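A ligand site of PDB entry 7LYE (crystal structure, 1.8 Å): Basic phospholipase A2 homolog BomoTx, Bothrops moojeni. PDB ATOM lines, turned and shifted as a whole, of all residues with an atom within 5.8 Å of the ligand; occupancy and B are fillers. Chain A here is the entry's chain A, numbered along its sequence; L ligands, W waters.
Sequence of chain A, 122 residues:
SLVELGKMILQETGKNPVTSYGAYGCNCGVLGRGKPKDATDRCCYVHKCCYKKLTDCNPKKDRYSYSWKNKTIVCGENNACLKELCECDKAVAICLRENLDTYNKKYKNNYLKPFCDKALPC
The backbone NH of Gly 29 lies close to a nitrogen (N2) of the ligand, 3.1 Å away. Merely in contact with the ligand: Leu 2, Leu 5, Gly 6, Ile 9, Pro 17, Val 18, Tyr 21, Cys 28, Val 30, Tyr 51, Lys 60 and Val 92. Hydrophobic or aromatic side chains within 4 Å of the ligand: Leu 5, Ile 9, Pro 17, Val 18, Tyr 21, His 47, Tyr 51 and Val 92. Of the 25 residues printed, 17 come within 4 Å of the ligand.
A ring nitrogen (ND1) of His 47 is in hydrogen-bond range of an oxygen (O5) of the ligand, at 2.7 Å. An oxygen (O2) of the ligand is in salt-bridge range of the side-chain amino group of Lys 48 (2.8 Å). N2 of the ligand sits at hydrogen-bond distance from O of Asn 27 (2.8 Å). The side-chain sulfur (SG) of Cys 44 lies close to a nitrogen (N2) of the ligand (3.7 Å).
The side-chain hydroxyl (OH) of Tyr 51 lies close to a ring nitrogen (NE2) of His 47, 3.4 Å away. The backbone carbonyl oxygen of Asn 27 lies within hydrogen-bond range of the side-chain amino group of Lys 48 (2.8 Å). The side-chain amino group of Lys 48 lies within hydrogen-bond range of the backbone carbonyl oxygen of Val 30. The side-chain sulfur of Cys 44 forms a disulfide with the side-chain sulfur of Cys 28. The backbone NH (N) of Leu 2 sits at hydrogen-bond distance from the backbone carbonyl oxygen (O) of Lys 60, at 3.2 Å. The backbone NH (N) of Gly 22 is in hydrogen-bond range of the backbone carbonyl oxygen (O) of Pro 17.
Water W1 bridges an oxygen (O2) of the ligand (2.8 Å) and the backbone NH (N) of Gly 32 (2.9 Å).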
ATOM      1  N   LEU A   2      12.355 -15.964 -20.528  1.00  0.00           N
ATOM      2  CA  LEU A   2      11.353 -15.564 -21.503  1.00  0.00           C
ATOM      3  C   LEU A   2      11.578 -14.149 -22.011  1.00  0.00           C
ATOM      4  O   LEU A   2      11.136 -13.822 -23.123  1.00  0.00           O
ATOM      5  CB  LEU A   2       9.958 -15.693 -20.898  1.00  0.00           C
ATOM      6  CG  LEU A   2       9.469 -17.125 -20.671  1.00  0.00           C
ATOM      7  CD1 LEU A   2       8.008 -17.140 -20.234  1.00  0.00           C
ATOM      8  CD2 LEU A   2       9.663 -17.963 -21.932  1.00  0.00           C
ATOM      9  N   VAL A   3      12.251 -13.303 -21.233  1.00  0.00           N
ATOM     10  CA  VAL A   3      12.525 -11.940 -21.670  1.00  0.00           C
ATOM     11  C   VAL A   3      13.459 -11.943 -22.877  1.00  0.00           C
ATOM     12  O   VAL A   3      13.224 -11.257 -23.872  1.00  0.00           O
ATOM     13  CB  VAL A   3      13.098 -11.104 -20.511  1.00  0.00           C
ATOM     14  CG1 VAL A   3      13.616  -9.772 -21.013  1.00  0.00           C
ATOM     15  CG2 VAL A   3      12.036 -10.894 -19.442  1.00  0.00           C
ATOM     16  N   LEU A   5      13.994 -14.577 -24.809  1.00  0.00           N
ATOM     17  CA  LEU A   5      13.337 -15.324 -25.870  1.00  0.00           C
ATOM     18  C   LEU A   5      12.395 -14.427 -26.669  1.00  0.00           C
ATOM     19  O   LEU A   5      12.419 -14.434 -27.912  1.00  0.00           O
ATOM     20  CB  LEU A   5      12.571 -16.512 -25.278  1.00  0.00           C
ATOM     21  CG  LEU A   5      11.675 -17.300 -26.237  1.00  0.00           C
ATOM     22  CD1 LEU A   5      12.488 -17.845 -27.400  1.00  0.00           C
ATOM     23  CD2 LEU A   5      10.955 -18.420 -25.496  1.00  0.00           C
ATOM     24  N   GLY A   6      11.586 -13.621 -25.976  1.00  0.00           N
ATOM     25  CA  GLY A   6      10.648 -12.759 -26.676  1.00  0.00           C
ATOM     26  C   GLY A   6      11.345 -11.717 -27.533  1.00  0.00           C
ATOM     27  O   GLY A   6      10.865 -11.361 -28.612  1.00  0.00           O
ATOM     28  N   LYS A   7      12.485 -11.210 -27.072  1.00  0.00           N
ATOM     29  CA  LYS A   7      13.226 -10.236 -27.849  1.00  0.00           C
ATOM     30  C   LYS A   7      13.813 -10.874 -29.111  1.00  0.00           C
ATOM     31  O   LYS A   7      13.783 -10.270 -30.189  1.00  0.00           O
ATOM     32  CB  LYS A   7      14.322  -9.597 -27.008  1.00  0.00           C
ATOM     33  CG  LYS A   7      14.963  -8.375 -27.647  1.00  0.00           C
ATOM     34  CD  LYS A   7      15.722  -7.554 -26.624  1.00  0.00           C
ATOM     35  CE  LYS A   7      16.247  -6.272 -27.244  1.00  0.00           C
ATOM     36  NZ  LYS A   7      15.288  -5.138 -27.125  1.00  0.00           N
ATOM     37  N   ILE A   9      12.540 -13.426 -30.766  1.00  0.00           N
ATOM     38  CA  ILE A   9      11.460 -13.697 -31.702  1.00  0.00           C
ATOM     39  C   ILE A   9      11.079 -12.427 -32.449  1.00  0.00           C
ATOM     40  O   ILE A   9      10.897 -12.426 -33.675  1.00  0.00           O
ATOM     41  CB  ILE A   9      10.255 -14.300 -30.967  1.00  0.00           C
ATOM     42  CG1 ILE A   9      10.617 -15.672 -30.395  1.00  0.00           C
ATOM     43  CG2 ILE A   9       9.051 -14.398 -31.895  1.00  0.00           C
ATOM     44  CD1 ILE A   9       9.462 -16.381 -29.739  1.00  0.00           C
ATOM     45  N   PRO A  17       5.849 -11.569 -29.966  1.00  0.00           N
ATOM     46  CA  PRO A  17       5.743 -12.982 -29.570  1.00  0.00           C
ATOM     47  C   PRO A  17       4.427 -13.336 -28.896  1.00  0.00           C
ATOM     48  O   PRO A  17       3.949 -14.460 -29.060  1.00  0.00           O
ATOM     49  CB  PRO A  17       6.930 -13.158 -28.610  1.00  0.00           C
ATOM     50  CG  PRO A  17       7.302 -11.770 -28.184  1.00  0.00           C
ATOM     51  CD  PRO A  17       7.010 -10.899 -29.364  1.00  0.00           C
ATOM     52  N   VAL A  18       3.824 -12.406 -28.161  1.00  0.00           N
ATOM     53  CA  VAL A  18       2.581 -12.710 -27.455  1.00  0.00           C
ATOM     54  C   VAL A  18       1.423 -12.830 -28.444  1.00  0.00           C
ATOM     55  O   VAL A  18       0.706 -13.843 -28.470  1.00  0.00           O
ATOM     56  CB  VAL A  18       2.288 -11.646 -26.387  1.00  0.00           C
ATOM     57  CG1 VAL A  18       0.887 -11.842 -25.815  1.00  0.00           C
ATOM     58  CG2 VAL A  18       3.335 -11.703 -25.278  1.00  0.00           C
ATOM     59  N   TYR A  21       2.418 -15.705 -31.240  1.00  0.00           N
ATOM     60  CA  TYR A  21       2.773 -17.050 -30.822  1.00  0.00           C
ATOM     61  C   TYR A  21       2.387 -17.381 -29.384  1.00  0.00           C
ATOM     62  O   TYR A  21       2.830 -18.407 -28.857  1.00  0.00           O
ATOM     63  CB  TYR A  21       4.291 -17.265 -30.990  1.00  0.00           C
ATOM     64  CG  TYR A  21       4.818 -17.048 -32.391  1.00  0.00           C
ATOM     65  CD1 TYR A  21       4.489 -17.911 -33.428  1.00  0.00           C
ATOM     66  CD2 TYR A  21       5.652 -15.973 -32.673  1.00  0.00           C
ATOM     67  CE1 TYR A  21       4.975 -17.719 -34.708  1.00  0.00           C
ATOM     68  CE2 TYR A  21       6.152 -15.771 -33.951  1.00  0.00           C
ATOM     69  CZ  TYR A  21       5.813 -16.644 -34.968  1.00  0.00           C
ATOM     70  OH  TYR A  21       6.294 -16.435 -36.242  1.00  0.00           O
ATOM     71  N   GLY A  22       1.570 -16.548 -28.727  1.00  0.00           N
ATOM     72  CA  GLY A  22       1.334 -16.738 -27.296  1.00  0.00           C
ATOM     73  C   GLY A  22       0.495 -17.957 -26.959  1.00  0.00           C
ATOM     74  O   GLY A  22       0.590 -18.479 -25.840  1.00  0.00           O
ATOM     75  N   ASN A  27       1.693 -26.400 -29.050  1.00  0.00           N
ATOM     76  CA  ASN A  27       2.968 -26.218 -28.369  1.00  0.00           C
ATOM     77  C   ASN A  27       3.349 -24.768 -28.133  1.00  0.00           C
ATOM     78  O   ASN A  27       3.912 -24.452 -27.072  1.00  0.00           O
ATOM     79  CB  ASN A  27       4.106 -26.906 -29.162  1.00  0.00           C
ATOM     80  CG  ASN A  27       3.896 -28.404 -29.300  1.00  0.00           C
ATOM     81  OD1 ASN A  27       4.369 -29.186 -28.477  1.00  0.00           O
ATOM     82  ND2 ASN A  27       3.191 -28.804 -30.352  1.00  0.00           N
ATOM     83  N   CYS A  28       3.082 -23.872 -29.086  1.00  0.00           N
ATOM     84  CA  CYS A  28       3.611 -22.516 -28.991  1.00  0.00           C
ATOM     85  C   CYS A  28       2.919 -21.730 -27.878  1.00  0.00           C
ATOM     86  O   CYS A  28       1.686 -21.596 -27.880  1.00  0.00           O
ATOM     87  CB  CYS A  28       3.443 -21.782 -30.316  1.00  0.00           C
ATOM     88  SG  CYS A  28       4.510 -22.374 -31.644  1.00  0.00           S
ATOM     89  N   GLY A  29       3.703 -21.224 -26.933  1.00  0.00           N
ATOM     90  CA  GLY A  29       3.195 -20.355 -25.891  1.00  0.00           C
ATOM     91  C   GLY A  29       2.323 -21.015 -24.836  1.00  0.00           C
ATOM     92  O   GLY A  29       1.842 -20.320 -23.935  1.00  0.00           O
ATOM     93  N   VAL A  30       2.095 -22.326 -24.926  1.00  0.00           N
ATOM     94  CA  VAL A  30       1.305 -23.034 -23.921  1.00  0.00           C
ATOM     95  C   VAL A  30       2.225 -23.979 -23.171  1.00  0.00           C
ATOM     96  O   VAL A  30       3.344 -24.277 -23.599  1.00  0.00           O
ATOM     97  CB  VAL A  30       0.130 -23.800 -24.550  1.00  0.00           C
ATOM     98  CG1 VAL A  30      -0.900 -22.830 -25.122  1.00  0.00           C
ATOM     99  CG2 VAL A  30       0.625 -24.753 -25.637  1.00  0.00           C
ATOM    100  N   LEU A  31       1.741 -24.460 -22.034  1.00  0.00           N
ATOM    101  CA  LEU A  31       2.501 -25.429 -21.242  1.00  0.00           C
ATOM    102  C   LEU A  31       2.345 -26.820 -21.833  1.00  0.00           C
ATOM    103  O   LEU A  31       1.238 -27.236 -22.210  1.00  0.00           O
ATOM    104  CB  LEU A  31       2.032 -25.425 -19.789  1.00  0.00           C
ATOM    105  CG  LEU A  31       1.998 -24.044 -19.106  1.00  0.00           C
ATOM    106  CD1 LEU A  31       1.680 -24.179 -17.631  1.00  0.00           C
ATOM    107  CD2 LEU A  31       3.316 -23.326 -19.314  1.00  0.00           C
ATOM    108  N   GLY A  32       3.451 -27.546 -21.911  1.00  0.00           N
ATOM    109  CA  GLY A  32       3.432 -28.932 -22.326  1.00  0.00           C
ATOM    110  C   GLY A  32       3.480 -29.094 -23.838  1.00  0.00           C
ATOM    111  O   GLY A  32       3.112 -28.209 -24.609  1.00  0.00           O
ATOM    112  N   CYS A  43       8.145 -25.965 -34.446  1.00  0.00           N
ATOM    113  CA  CYS A  43       9.263 -25.206 -33.889  1.00  0.00           C
ATOM    114  C   CYS A  43       9.183 -25.150 -32.368  1.00  0.00           C
ATOM    115  O   CYS A  43      10.191 -25.317 -31.672  1.00  0.00           O
ATOM    116  CB  CYS A  43       9.279 -23.788 -34.446  1.00  0.00           C
ATOM    117  SG  CYS A  43       9.495 -23.614 -36.227  1.00  0.00           S
ATOM    118  N   CYS A  44       7.977 -24.911 -31.833  1.00  0.00           N
ATOM    119  CA  CYS A  44       7.815 -24.805 -30.395  1.00  0.00           C
ATOM    120  C   CYS A  44       7.893 -26.157 -29.715  1.00  0.00           C
ATOM    121  O   CYS A  44       8.371 -26.250 -28.575  1.00  0.00           O
ATOM    122  CB  CYS A  44       6.472 -24.136 -30.101  1.00  0.00           C
ATOM    123  SG  CYS A  44       6.377 -22.481 -30.818  1.00  0.00           S
ATOM    124  N   TYR A  45       7.436 -27.220 -30.380  1.00  0.00           N
ATOM    125  CA  TYR A  45       7.619 -28.560 -29.859  1.00  0.00           C
ATOM    126  C   TYR A  45       9.097 -28.898 -29.713  1.00  0.00           C
ATOM    127  O   TYR A  45       9.541 -29.386 -28.669  1.00  0.00           O
ATOM    128  CB  TYR A  45       6.924 -29.570 -30.779  1.00  0.00           C
ATOM    129  CG  TYR A  45       7.318 -31.010 -30.524  1.00  0.00           C
ATOM    130  CD1 TYR A  45       6.699 -31.746 -29.525  1.00  0.00           C
ATOM    131  CD2 TYR A  45       8.317 -31.620 -31.277  1.00  0.00           C
ATOM    132  CE1 TYR A  45       7.057 -33.063 -29.276  1.00  0.00           C
ATOM    133  CE2 TYR A  45       8.685 -32.931 -31.034  1.00  0.00           C
ATOM    134  CZ  TYR A  45       8.051 -33.645 -30.042  1.00  0.00           C
ATOM    135  OH  TYR A  45       8.411 -34.953 -29.799  1.00  0.00           O
ATOM    136  N   HIS A  47      11.546 -26.795 -29.522  1.00  0.00           N
ATOM    137  CA  HIS A  47      12.075 -25.903 -28.484  1.00  0.00           C
ATOM    138  C   HIS A  47      11.785 -26.445 -27.085  1.00  0.00           C
ATOM    139  O   HIS A  47      12.645 -26.407 -26.200  1.00  0.00           O
ATOM    140  CB  HIS A  47      11.473 -24.513 -28.679  1.00  0.00           C
ATOM    141  CG  HIS A  47      11.946 -23.505 -27.684  1.00  0.00           C
ATOM    142  ND1 HIS A  47      11.135 -23.002 -26.689  1.00  0.00           N
ATOM    143  CD2 HIS A  47      13.135 -22.879 -27.540  1.00  0.00           C
ATOM    144  CE1 HIS A  47      11.798 -22.120 -25.974  1.00  0.00           C
ATOM    145  NE2 HIS A  47      13.021 -22.020 -26.471  1.00  0.00           N
ATOM    146  N   LYS A  48      10.574 -26.965 -26.865  1.00  0.00           N
ATOM    147  CA  LYS A  48      10.248 -27.537 -25.567  1.00  0.00           C
ATOM    148  C   LYS A  48      11.093 -28.774 -25.287  1.00  0.00           C
ATOM    149  O   LYS A  48      11.490 -29.025 -24.142  1.00  0.00           O
ATOM    150  CB  LYS A  48       8.763 -27.874 -25.494  1.00  0.00           C
ATOM    151  CG  LYS A  48       7.895 -26.669 -25.147  1.00  0.00           C
ATOM    152  CD  LYS A  48       6.491 -26.826 -25.693  1.00  0.00           C
ATOM    153  CE  LYS A  48       5.485 -26.109 -24.805  1.00  0.00           C
ATOM    154  NZ  LYS A  48       5.636 -24.618 -24.880  1.00  0.00           N
ATOM    155  N   TYR A  51      14.392 -27.467 -24.084  1.00  0.00           N
ATOM    156  CA  TYR A  51      14.351 -27.095 -22.674  1.00  0.00           C
ATOM    157  C   TYR A  51      14.434 -28.315 -21.771  1.00  0.00           C
ATOM    158  O   TYR A  51      14.973 -28.236 -20.660  1.00  0.00           O
ATOM    159  CB  TYR A  51      13.065 -26.316 -22.375  1.00  0.00           C
ATOM    160  CG  TYR A  51      13.143 -24.832 -22.623  1.00  0.00           C
ATOM    161  CD1 TYR A  51      14.183 -24.277 -23.359  1.00  0.00           C
ATOM    162  CD2 TYR A  51      12.168 -23.977 -22.125  1.00  0.00           C
ATOM    163  CE1 TYR A  51      14.244 -22.922 -23.591  1.00  0.00           C
ATOM    164  CE2 TYR A  51      12.222 -22.614 -22.347  1.00  0.00           C
ATOM    165  CZ  TYR A  51      13.264 -22.093 -23.078  1.00  0.00           C
ATOM    166  OH  TYR A  51      13.326 -20.742 -23.297  1.00  0.00           O
ATOM    167  N   LYS A  60      12.925 -20.934 -18.186  1.00  0.00           N
ATOM    168  CA  LYS A  60      11.990 -19.818 -18.265  1.00  0.00           C
ATOM    169  C   LYS A  60      12.452 -18.623 -17.437  1.00  0.00           C
ATOM    170  O   LYS A  60      12.112 -17.477 -17.767  1.00  0.00           O
ATOM    171  CB  LYS A  60      10.598 -20.252 -17.830  1.00  0.00           C
ATOM    172  CG  LYS A  60       9.826 -21.042 -18.864  1.00  0.00           C
ATOM    173  CD  LYS A  60       8.650 -21.769 -18.227  1.00  0.00           C
ATOM    174  CE  LYS A  60       7.602 -22.128 -19.257  1.00  0.00           C
ATOM    175  NZ  LYS A  60       6.243 -22.137 -18.656  1.00  0.00           N
ATOM    176  N   VAL A  92      14.670 -21.542 -31.902  1.00  0.00           N
ATOM    177  CA  VAL A  92      13.235 -21.433 -32.118  1.00  0.00           C
ATOM    178  C   VAL A  92      12.893 -20.113 -32.788  1.00  0.00           C
ATOM    179  O   VAL A  92      11.960 -20.049 -33.608  1.00  0.00           O
ATOM    180  CB  VAL A  92      12.457 -21.632 -30.797  1.00  0.00           C
ATOM    181  CG1 VAL A  92      12.490 -20.370 -29.932  1.00  0.00           C
ATOM    182  CG2 VAL A  92      11.012 -22.019 -31.089  1.00  0.00           C
ATOM    183  N   LEU A  96      10.910 -20.112 -36.293  1.00  0.00           N
ATOM    184  CA  LEU A  96       9.654 -19.414 -36.492  1.00  0.00           C
ATOM    185  C   LEU A  96       9.722 -18.465 -37.691  1.00  0.00           C
ATOM    186  O   LEU A  96       8.761 -18.380 -38.465  1.00  0.00           O
ATOM    187  CB  LEU A  96       9.267 -18.648 -35.223  1.00  0.00           C
ATOM    188  CG  LEU A  96       8.877 -19.533 -34.033  1.00  0.00           C
ATOM    189  CD1 LEU A  96       8.712 -18.708 -32.763  1.00  0.00           C
ATOM    190  CD2 LEU A  96       7.617 -20.341 -34.328  1.00  0.00           C
HETATM  191  C1  LIG L   1       6.386 -19.368 -29.334  1.00  0.00           C
HETATM  192  C2  LIG L   1       6.878 -18.365 -28.284  1.00  0.00           C
HETATM  193  C3  LIG L   1       6.779 -18.934 -26.839  1.00  0.00           C
HETATM  194  C4  LIG L   1       7.331 -20.139 -26.395  1.00  0.00           C
HETATM  195  C5  LIG L   1       6.984 -20.240 -25.034  1.00  0.00           C
HETATM  196  C6  LIG L   1       6.257 -19.106 -24.732  1.00  0.00           C
HETATM  197  C7  LIG L   1       5.445 -17.055 -25.915  1.00  0.00           C
HETATM  198  C8  LIG L   1       6.386 -15.910 -25.433  1.00  0.00           C
HETATM  199  C9  LIG L   1       7.717 -16.171 -25.172  1.00  0.00           C
HETATM  200  C10 LIG L   1       8.559 -15.150 -24.732  1.00  0.00           C
HETATM  201  C11 LIG L   1       8.046 -13.875 -24.554  1.00  0.00           C
HETATM  202  C12 LIG L   1       6.706 -13.611 -24.813  1.00  0.00           C
HETATM  203  C13 LIG L   1       5.876 -14.627 -25.259  1.00  0.00           C
HETATM  204  C14 LIG L   1       5.759 -18.913 -23.429  1.00  0.00           C
HETATM  205  C15 LIG L   1       6.006 -19.857 -22.444  1.00  0.00           C
HETATM  206  C16 LIG L   1       6.738 -21.007 -22.750  1.00  0.00           C
HETATM  207  C17 LIG L   1       7.229 -21.205 -24.025  1.00  0.00           C
HETATM  208  C18 LIG L   1       8.918 -22.736 -23.339  1.00  0.00           C
HETATM  209  C19 LIG L   1       8.333 -23.798 -22.415  1.00  0.00           C
HETATM  210  C20 LIG L   1       8.133 -21.160 -27.231  1.00  0.00           C
HETATM  211  C21 LIG L   1       7.701 -22.619 -27.185  1.00  0.00           C
HETATM  212  N1  LIG L   1       6.152 -18.351 -25.841  1.00  0.00           N
HETATM  213  N2  LIG L   1       6.279 -22.898 -27.094  1.00  0.00           N
HETATM  214  O1  LIG L   1       7.976 -22.378 -24.324  1.00  0.00           O
HETATM  215  O2  LIG L   1       7.211 -24.301 -22.647  1.00  0.00           O
HETATM  216  O3  LIG L   1       9.001 -24.164 -21.405  1.00  0.00           O
HETATM  217  O4  LIG L   1       9.041 -20.819 -27.915  1.00  0.00           O
HETATM  218  O5  LIG L   1       8.502 -23.497 -27.211  1.00  0.00           O
HETATM  219  O   HOH W   1       6.052 -26.392 -21.232  1.00  0.00           O
HETATM  220  O   HOH W   2       9.770 -26.475 -20.175  1.00  0.00           O
